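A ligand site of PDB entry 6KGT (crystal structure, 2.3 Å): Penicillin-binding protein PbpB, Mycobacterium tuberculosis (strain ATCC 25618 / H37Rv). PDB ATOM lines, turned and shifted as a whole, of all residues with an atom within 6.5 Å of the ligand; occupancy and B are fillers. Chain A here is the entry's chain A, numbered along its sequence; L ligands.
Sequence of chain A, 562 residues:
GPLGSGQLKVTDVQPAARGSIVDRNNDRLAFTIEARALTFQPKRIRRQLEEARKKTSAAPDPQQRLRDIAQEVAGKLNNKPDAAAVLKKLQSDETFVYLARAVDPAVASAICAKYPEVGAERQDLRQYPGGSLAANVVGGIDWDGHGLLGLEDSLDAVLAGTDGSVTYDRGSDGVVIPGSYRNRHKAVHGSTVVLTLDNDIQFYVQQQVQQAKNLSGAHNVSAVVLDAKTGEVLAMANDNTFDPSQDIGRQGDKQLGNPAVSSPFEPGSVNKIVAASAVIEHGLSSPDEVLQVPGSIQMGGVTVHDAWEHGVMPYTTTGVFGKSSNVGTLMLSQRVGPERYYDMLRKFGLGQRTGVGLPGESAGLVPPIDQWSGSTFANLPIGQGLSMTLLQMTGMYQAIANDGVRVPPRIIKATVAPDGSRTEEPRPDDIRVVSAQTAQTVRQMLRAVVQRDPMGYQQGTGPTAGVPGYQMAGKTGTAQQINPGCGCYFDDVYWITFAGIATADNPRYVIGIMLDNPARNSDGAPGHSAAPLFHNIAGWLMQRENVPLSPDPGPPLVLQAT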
ATOM      1  N   PRO A 267      27.682  11.749  26.395  1.00  0.00           N
ATOM      2  CA  PRO A 267      26.906  11.847  25.160  1.00  0.00           C
ATOM      3  C   PRO A 267      26.476  13.252  24.795  1.00  0.00           C
ATOM      4  O   PRO A 267      26.167  13.504  23.611  1.00  0.00           O
ATOM      5  CB  PRO A 267      25.675  10.990  25.460  1.00  0.00           C
ATOM      6  CG  PRO A 267      25.495  11.203  26.995  1.00  0.00           C
ATOM      7  CD  PRO A 267      26.893  11.178  27.509  1.00  0.00           C
ATOM      8  N   GLY A 268      26.422  14.171  25.752  1.00  0.00           N
ATOM      9  CA  GLY A 268      25.884  15.477  25.453  1.00  0.00           C
ATOM     10  C   GLY A 268      24.426  15.402  25.084  1.00  0.00           C
ATOM     11  O   GLY A 268      23.694  14.475  25.478  1.00  0.00           O
ATOM     12  N   SER A 269      23.986  16.371  24.284  1.00  0.00           N
ATOM     13  CA  SER A 269      22.561  16.534  24.005  1.00  0.00           C
ATOM     14  C   SER A 269      21.896  15.323  23.354  1.00  0.00           C
ATOM     15  O   SER A 269      20.656  15.222  23.386  1.00  0.00           O
ATOM     16  CB  SER A 269      22.368  17.764  23.106  1.00  0.00           C
ATOM     17  OG  SER A 269      22.801  18.907  23.792  1.00  0.00           O
ATOM     18  N   VAL A 270      22.660  14.393  22.746  1.00  0.00           N
ATOM     19  CA  VAL A 270      22.014  13.166  22.271  1.00  0.00           C
ATOM     20  C   VAL A 270      21.306  12.440  23.423  1.00  0.00           C
ATOM     21  O   VAL A 270      20.307  11.738  23.198  1.00  0.00           O
ATOM     22  CB  VAL A 270      23.040  12.276  21.532  1.00  0.00           C
ATOM     23  CG1 VAL A 270      22.536  10.888  21.338  1.00  0.00           C
ATOM     24  CG2 VAL A 270      23.339  12.856  20.186  1.00  0.00           C
ATOM     25  N   LYS A 272      19.294  13.690  25.377  1.00  0.00           N
ATOM     26  CA  LYS A 272      18.001  14.288  25.675  1.00  0.00           C
ATOM     27  C   LYS A 272      16.821  13.426  25.243  1.00  0.00           C
ATOM     28  O   LYS A 272      15.687  13.738  25.605  1.00  0.00           O
ATOM     29  CB  LYS A 272      17.950  15.676  25.027  1.00  0.00           C
ATOM     30  CG  LYS A 272      18.935  16.665  25.677  1.00  0.00           C
ATOM     31  CD  LYS A 272      18.794  18.064  25.085  1.00  0.00           C
ATOM     32  CE  LYS A 272      19.758  19.089  25.731  1.00  0.00           C
ATOM     33  NZ  LYS A 272      19.736  20.389  24.969  1.00  0.00           N
ATOM     34  N   HIS A 305      23.097  27.494  31.192  1.00  0.00           N
ATOM     35  CA  HIS A 305      22.820  28.417  30.105  1.00  0.00           C
ATOM     36  C   HIS A 305      22.518  27.618  28.842  1.00  0.00           C
ATOM     37  O   HIS A 305      22.978  26.489  28.688  1.00  0.00           O
ATOM     38  CB  HIS A 305      24.018  29.353  29.869  1.00  0.00           C
ATOM     39  CG  HIS A 305      25.359  28.670  29.714  1.00  0.00           C
ATOM     40  ND1 HIS A 305      25.713  27.527  30.404  1.00  0.00           N
ATOM     41  CD2 HIS A 305      26.423  28.976  28.936  1.00  0.00           C
ATOM     42  CE1 HIS A 305      26.944  27.160  30.069  1.00  0.00           C
ATOM     43  NE2 HIS A 305      27.393  28.028  29.174  1.00  0.00           N
ATOM     44  N   ASP A 306      21.740  28.207  27.947  1.00  0.00           N
ATOM     45  CA  ASP A 306      21.633  27.681  26.607  1.00  0.00           C
ATOM     46  C   ASP A 306      22.842  28.137  25.798  1.00  0.00           C
ATOM     47  O   ASP A 306      23.423  29.198  26.055  1.00  0.00           O
ATOM     48  CB  ASP A 306      20.324  28.139  25.943  1.00  0.00           C
ATOM     49  CG  ASP A 306      19.110  27.358  26.435  1.00  0.00           C
ATOM     50  OD1 ASP A 306      19.304  26.407  27.235  1.00  0.00           O
ATOM     51  OD2 ASP A 306      17.974  27.668  26.017  1.00  0.00           O
ATOM     52  N   ALA A 307      23.222  27.325  24.800  1.00  0.00           N
ATOM     53  CA  ALA A 307      24.429  27.565  24.007  1.00  0.00           C
ATOM     54  C   ALA A 307      24.331  28.823  23.143  1.00  0.00           C
ATOM     55  O   ALA A 307      25.240  29.135  22.361  1.00  0.00           O
ATOM     56  CB  ALA A 307      24.725  26.360  23.118  1.00  0.00           C
ATOM     57  N   TRP A 308      23.215  29.545  23.253  1.00  0.00           N
ATOM     58  CA  TRP A 308      23.035  30.840  22.618  1.00  0.00           C
ATOM     59  C   TRP A 308      22.345  31.727  23.644  1.00  0.00           C
ATOM     60  O   TRP A 308      21.571  31.227  24.465  1.00  0.00           O
ATOM     61  CB  TRP A 308      22.215  30.754  21.310  1.00  0.00           C
ATOM     62  CG  TRP A 308      20.767  30.229  21.463  1.00  0.00           C
ATOM     63  CD1 TRP A 308      19.618  30.961  21.354  1.00  0.00           C
ATOM     64  CD2 TRP A 308      20.349  28.866  21.718  1.00  0.00           C
ATOM     65  NE1 TRP A 308      18.513  30.157  21.541  1.00  0.00           N
ATOM     66  CE2 TRP A 308      18.932  28.869  21.769  1.00  0.00           C
ATOM     67  CE3 TRP A 308      21.031  27.659  21.926  1.00  0.00           C
ATOM     68  CZ2 TRP A 308      18.188  27.699  22.006  1.00  0.00           C
ATOM     69  CZ3 TRP A 308      20.278  26.501  22.171  1.00  0.00           C
ATOM     70  CH2 TRP A 308      18.881  26.531  22.205  1.00  0.00           C
ATOM     71  N   GLY A 322      14.305  20.199  19.369  1.00  0.00           N
ATOM     72  CA  GLY A 322      14.775  20.541  18.027  1.00  0.00           C
ATOM     73  C   GLY A 322      15.867  21.594  18.023  1.00  0.00           C
ATOM     74  O   GLY A 322      16.802  21.530  17.225  1.00  0.00           O
ATOM     75  N   LYS A 323      15.757  22.579  18.909  1.00  0.00           N
ATOM     76  CA  LYS A 323      16.803  23.589  19.061  1.00  0.00           C
ATOM     77  C   LYS A 323      17.849  23.222  20.105  1.00  0.00           C
ATOM     78  O   LYS A 323      18.872  23.889  20.203  1.00  0.00           O
ATOM     79  CB  LYS A 323      16.180  24.951  19.395  1.00  0.00           C
ATOM     80  CG  LYS A 323      15.620  25.635  18.158  1.00  0.00           C
ATOM     81  CD  LYS A 323      14.746  26.810  18.476  1.00  0.00           C
ATOM     82  CE  LYS A 323      13.952  27.221  17.239  1.00  0.00           C
ATOM     83  NZ  LYS A 323      14.783  27.403  16.001  1.00  0.00           N
ATOM     84  N   SER A 324      17.605  22.152  20.857  1.00  0.00           N
ATOM     85  CA  SER A 324      18.494  21.658  21.909  1.00  0.00           C
ATOM     86  C   SER A 324      18.727  22.732  22.991  1.00  0.00           C
ATOM     87  O   SER A 324      19.863  23.112  23.298  1.00  0.00           O
ATOM     88  CB  SER A 324      19.795  21.143  21.317  1.00  0.00           C
ATOM     89  OG  SER A 324      20.346  20.157  22.176  1.00  0.00           O
ATOM     90  N   SER A 325      17.624  23.189  23.567  1.00  0.00           N
ATOM     91  CA  SER A 325      17.663  24.104  24.702  1.00  0.00           C
ATOM     92  C   SER A 325      17.944  23.344  25.997  1.00  0.00           C
ATOM     93  O   SER A 325      17.148  22.493  26.388  1.00  0.00           O
ATOM     94  CB  SER A 325      16.332  24.858  24.775  1.00  0.00           C
ATOM     95  OG  SER A 325      16.172  25.533  25.997  1.00  0.00           O
ATOM     96  N   ASN A 326      19.092  23.614  26.624  1.00  0.00           N
ATOM     97  CA  ASN A 326      19.396  23.044  27.937  1.00  0.00           C
ATOM     98  C   ASN A 326      18.348  23.452  28.970  1.00  0.00           C
ATOM     99  O   ASN A 326      17.826  22.603  29.710  1.00  0.00           O
ATOM    100  CB  ASN A 326      20.783  23.495  28.405  1.00  0.00           C
ATOM    101  CG  ASN A 326      21.892  22.854  27.592  1.00  0.00           C
ATOM    102  OD1 ASN A 326      21.674  21.833  26.927  1.00  0.00           O
ATOM    103  ND2 ASN A 326      23.095  23.447  27.630  1.00  0.00           N
ATOM    104  N   ILE A 382      21.047  16.724  30.188  1.00  0.00           N
ATOM    105  CA  ILE A 382      21.646  17.312  28.992  1.00  0.00           C
ATOM    106  C   ILE A 382      22.872  16.536  28.527  1.00  0.00           C
ATOM    107  O   ILE A 382      23.512  16.926  27.536  1.00  0.00           O
ATOM    108  CB  ILE A 382      21.985  18.802  29.197  1.00  0.00           C
ATOM    109  CG1 ILE A 382      23.029  18.990  30.315  1.00  0.00           C
ATOM    110  CG2 ILE A 382      20.705  19.602  29.521  1.00  0.00           C
ATOM    111  CD1 ILE A 382      23.390  20.433  30.565  1.00  0.00           C
ATOM    112  N   GLY A 383      23.188  15.433  29.189  1.00  0.00           N
ATOM    113  CA  GLY A 383      24.206  14.544  28.683  1.00  0.00           C
ATOM    114  C   GLY A 383      25.606  14.723  29.232  1.00  0.00           C
ATOM    115  O   GLY A 383      26.541  14.226  28.609  1.00  0.00           O
ATOM    116  N   GLN A 384      25.794  15.428  30.357  1.00  0.00           N
ATOM    117  CA  GLN A 384      27.088  15.477  31.034  1.00  0.00           C
ATOM    118  C   GLN A 384      26.942  14.809  32.398  1.00  0.00           C
ATOM    119  O   GLN A 384      25.847  14.739  32.961  1.00  0.00           O
ATOM    120  CB  GLN A 384      27.622  16.921  31.191  1.00  0.00           C
ATOM    121  CG  GLN A 384      27.744  17.738  29.879  1.00  0.00           C
ATOM    122  CD  GLN A 384      29.128  17.658  29.115  1.00  0.00           C
ATOM    123  OE1 GLN A 384      29.399  18.517  28.273  1.00  0.00           O
ATOM    124  NE2 GLN A 384      29.968  16.648  29.414  1.00  0.00           N
ATOM    125  N   VAL A 449      14.624  18.185  14.574  1.00  0.00           N
ATOM    126  CA  VAL A 449      16.071  18.411  14.551  1.00  0.00           C
ATOM    127  C   VAL A 449      16.583  18.559  13.110  1.00  0.00           C
ATOM    128  O   VAL A 449      17.532  19.320  12.858  1.00  0.00           O
ATOM    129  CB  VAL A 449      16.790  17.252  15.281  1.00  0.00           C
ATOM    130  CG1 VAL A 449      18.288  17.394  15.148  1.00  0.00           C
ATOM    131  CG2 VAL A 449      16.343  17.180  16.751  1.00  0.00           C
ATOM    132  N   THR A 461      18.684  21.901  14.867  1.00  0.00           N
ATOM    133  CA  THR A 461      20.141  21.969  14.932  1.00  0.00           C
ATOM    134  C   THR A 461      20.823  21.136  13.842  1.00  0.00           C
ATOM    135  O   THR A 461      22.020  21.342  13.606  1.00  0.00           O
ATOM    136  CB  THR A 461      20.616  21.500  16.301  1.00  0.00           C
ATOM    137  OG1 THR A 461      20.143  20.171  16.557  1.00  0.00           O
ATOM    138  CG2 THR A 461      20.124  22.451  17.419  1.00  0.00           C
ATOM    139  N   GLY A 462      20.110  20.225  13.174  1.00  0.00           N
ATOM    140  CA  GLY A 462      20.761  19.305  12.263  1.00  0.00           C
ATOM    141  C   GLY A 462      20.083  19.174  10.919  1.00  0.00           C
ATOM    142  O   GLY A 462      19.808  18.062  10.450  1.00  0.00           O
ATOM    143  N   LYS A 475      19.087  13.306  16.656  1.00  0.00           N
ATOM    144  CA  LYS A 475      19.484  14.300  17.645  1.00  0.00           C
ATOM    145  C   LYS A 475      20.983  14.545  17.529  1.00  0.00           C
ATOM    146  O   LYS A 475      21.767  13.595  17.381  1.00  0.00           O
ATOM    147  CB  LYS A 475      19.098  13.844  19.065  1.00  0.00           C
ATOM    148  CG  LYS A 475      19.370  14.878  20.164  1.00  0.00           C
ATOM    149  CD  LYS A 475      18.472  16.126  20.000  1.00  0.00           C
ATOM    150  CE  LYS A 475      18.885  17.251  20.958  1.00  0.00           C
ATOM    151  NZ  LYS A 475      20.055  18.043  20.437  1.00  0.00           N
ATOM    152  N   THR A 476      21.372  15.819  17.555  1.00  0.00           N
ATOM    153  CA  THR A 476      22.765  16.274  17.507  1.00  0.00           C
ATOM    154  C   THR A 476      23.343  16.377  18.907  1.00  0.00           C
ATOM    155  O   THR A 476      22.621  16.583  19.887  1.00  0.00           O
ATOM    156  CB  THR A 476      22.861  17.647  16.834  1.00  0.00           C
ATOM    157  OG1 THR A 476      21.815  18.482  17.367  1.00  0.00           O
ATOM    158  CG2 THR A 476      22.730  17.541  15.315  1.00  0.00           C
ATOM    159  N   GLY A 477      24.656  16.264  19.004  1.00  0.00           N
ATOM    160  CA  GLY A 477      25.276  16.378  20.298  1.00  0.00           C
ATOM    161  C   GLY A 477      26.659  16.990  20.284  1.00  0.00           C
ATOM    162  O   GLY A 477      27.461  16.774  19.378  1.00  0.00           O
ATOM    163  N   THR A 478      26.923  17.717  21.361  1.00  0.00           N
ATOM    164  CA  THR A 478      28.232  18.313  21.639  1.00  0.00           C
ATOM    165  C   THR A 478      28.449  18.162  23.139  1.00  0.00           C
ATOM    166  O   THR A 478      27.632  18.620  23.934  1.00  0.00           O
ATOM    167  CB  THR A 478      28.246  19.795  21.233  1.00  0.00           C
ATOM    168  OG1 THR A 478      27.969  19.897  19.826  1.00  0.00           O
ATOM    169  CG2 THR A 478      29.587  20.404  21.516  1.00  0.00           C
ATOM    170  N   ALA A 479      29.544  17.491  23.531  1.00  0.00           N
ATOM    171  CA  ALA A 479      29.835  17.283  24.944  1.00  0.00           C
ATOM    172  C   ALA A 479      31.290  17.617  25.213  1.00  0.00           C
ATOM    173  O   ALA A 479      32.192  17.138  24.503  1.00  0.00           O
ATOM    174  CB  ALA A 479      29.536  15.838  25.363  1.00  0.00           C
ATOM    175  N   THR A 497      28.360  14.002  18.583  1.00  0.00           N
ATOM    176  CA  THR A 497      27.535  12.803  18.524  1.00  0.00           C
ATOM    177  C   THR A 497      26.323  13.075  17.638  1.00  0.00           C
ATOM    178  O   THR A 497      25.846  14.210  17.536  1.00  0.00           O
ATOM    179  CB  THR A 497      27.004  12.372  19.909  1.00  0.00           C
ATOM    180  OG1 THR A 497      26.417  13.505  20.570  1.00  0.00           O
ATOM    181  CG2 THR A 497      28.117  11.805  20.768  1.00  0.00           C
HETATM  182  C1  LIG L   1      23.968  19.326  23.606  1.00  0.00           C
HETATM  183  C2  LIG L   1      24.226  20.846  23.776  1.00  0.00           C
HETATM  184  N1  LIG L   1      23.245  20.685  21.542  1.00  0.00           N
HETATM  185  C3  LIG L   1      23.293  21.513  22.924  1.00  0.00           C
HETATM  186  C4  LIG L   1      23.844  21.570  20.458  1.00  0.00           C
HETATM  187  C5  LIG L   1      24.281  22.961  20.986  1.00  0.00           C
HETATM  188  S1  LIG L   1      23.929  23.062  22.456  1.00  0.00           S
HETATM  189  C6  LIG L   1      23.820  21.024  19.031  1.00  0.00           C
HETATM  190  O1  LIG L   1      24.884  18.625  23.108  1.00  0.00           O
HETATM  191  C7  LIG L   1      24.057  21.283  25.267  1.00  0.00           C
HETATM  192  O2  LIG L   1      24.402  22.618  25.396  1.00  0.00           O
HETATM  193  C8  LIG L   1      24.923  20.446  26.204  1.00  0.00           C
HETATM  194  C9  LIG L   1      24.256  24.322  20.273  1.00  0.00           C
HETATM  195  C10 LIG L   1      25.413  24.685  19.762  1.00  0.00           C
HETATM  196  C11 LIG L   1      25.019  26.105  19.088  1.00  0.00           C
HETATM  197  C12 LIG L   1      23.763  25.941  18.573  1.00  0.00           C
HETATM  198  O3  LIG L   1      23.254  24.578  19.056  1.00  0.00           O
HETATM  199  O4  LIG L   1      24.737  21.243  18.192  1.00  0.00           O
HETATM  200  O5  LIG L   1      22.844  20.307  18.709  1.00  0.00           O
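The backbone NH (N) of Ser 269 lies close to an oxygen (O1) of the ligand (2.7 Å).
C1 of the ligand is covalently linked to OG of Ser 269 (1.3 Å).
OG1 of Thr 476 sits at hydrogen-bond distance from O5 of the ligand.
ND2 of Asn 326 sits at hydrogen-bond distance from O2 of the ligand (2.7 Å).
The backbone NH (N) of Thr 478 sits at hydrogen-bond distance from an oxygen (O1) of the ligand.
A nitrogen (N1) of the ligand lies within hydrogen-bond range of the side-chain hydroxyl (OG) of Ser 324 (3.0 Å).
OG1 of Thr 461 is in hydrogen-bond range of O5 of the ligand (3.5 Å).
NZ of Lys 475 lies within salt-bridge range of O5 of the ligand.
OG1 of Thr 476 sits at hydrogen-bond distance from OG1 of Thr 461 (2.5 Å).
OD1 of Asn 326 sits at hydrogen-bond distance from NZ of Lys 272 (3.1 Å).
The side-chain amide nitrogen of Asn 326 sits at hydrogen-bond distance from the backbone carbonyl oxygen of His 305, 3.2 Å away.
The backbone NH of Asn 326 lies within hydrogen-bond range of the side-chain carboxylate of Asp 306 (2.9 Å).
The side-chain amino group (NZ) of Lys 475 lies within hydrogen-bond range of the side-chain hydroxyl (OG) of Ser 324, 2.8 Å away.
N of Thr 461 sits at hydrogen-bond distance from O of Val 449, at 3.5 Å.
N of Gly 477 sits at hydrogen-bond distance from O of Thr 497, 2.8 Å away.
The backbone carbonyl oxygen of Gly 383 sits at hydrogen-bond distance from the backbone NH of Gly 268 (2.9 Å).
Gly 268 touches the ligand (C to O1, 3.8 Å).
CB of Ala 307 touches S1 of the ligand, 3.5 Å away.
Gly 477 touches the ligand (CA to O1, 3.6 Å).
Hydrophobic or aromatic side chains that line the ligand: Ala 307.
Ten residues have an atom within 4 Å of the ligand: Gly 268, Ser 269, Ala 307, Ser 324, Asn 326, Thr 461, Lys 475, Thr 476, Gly 477 and Thr 478.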
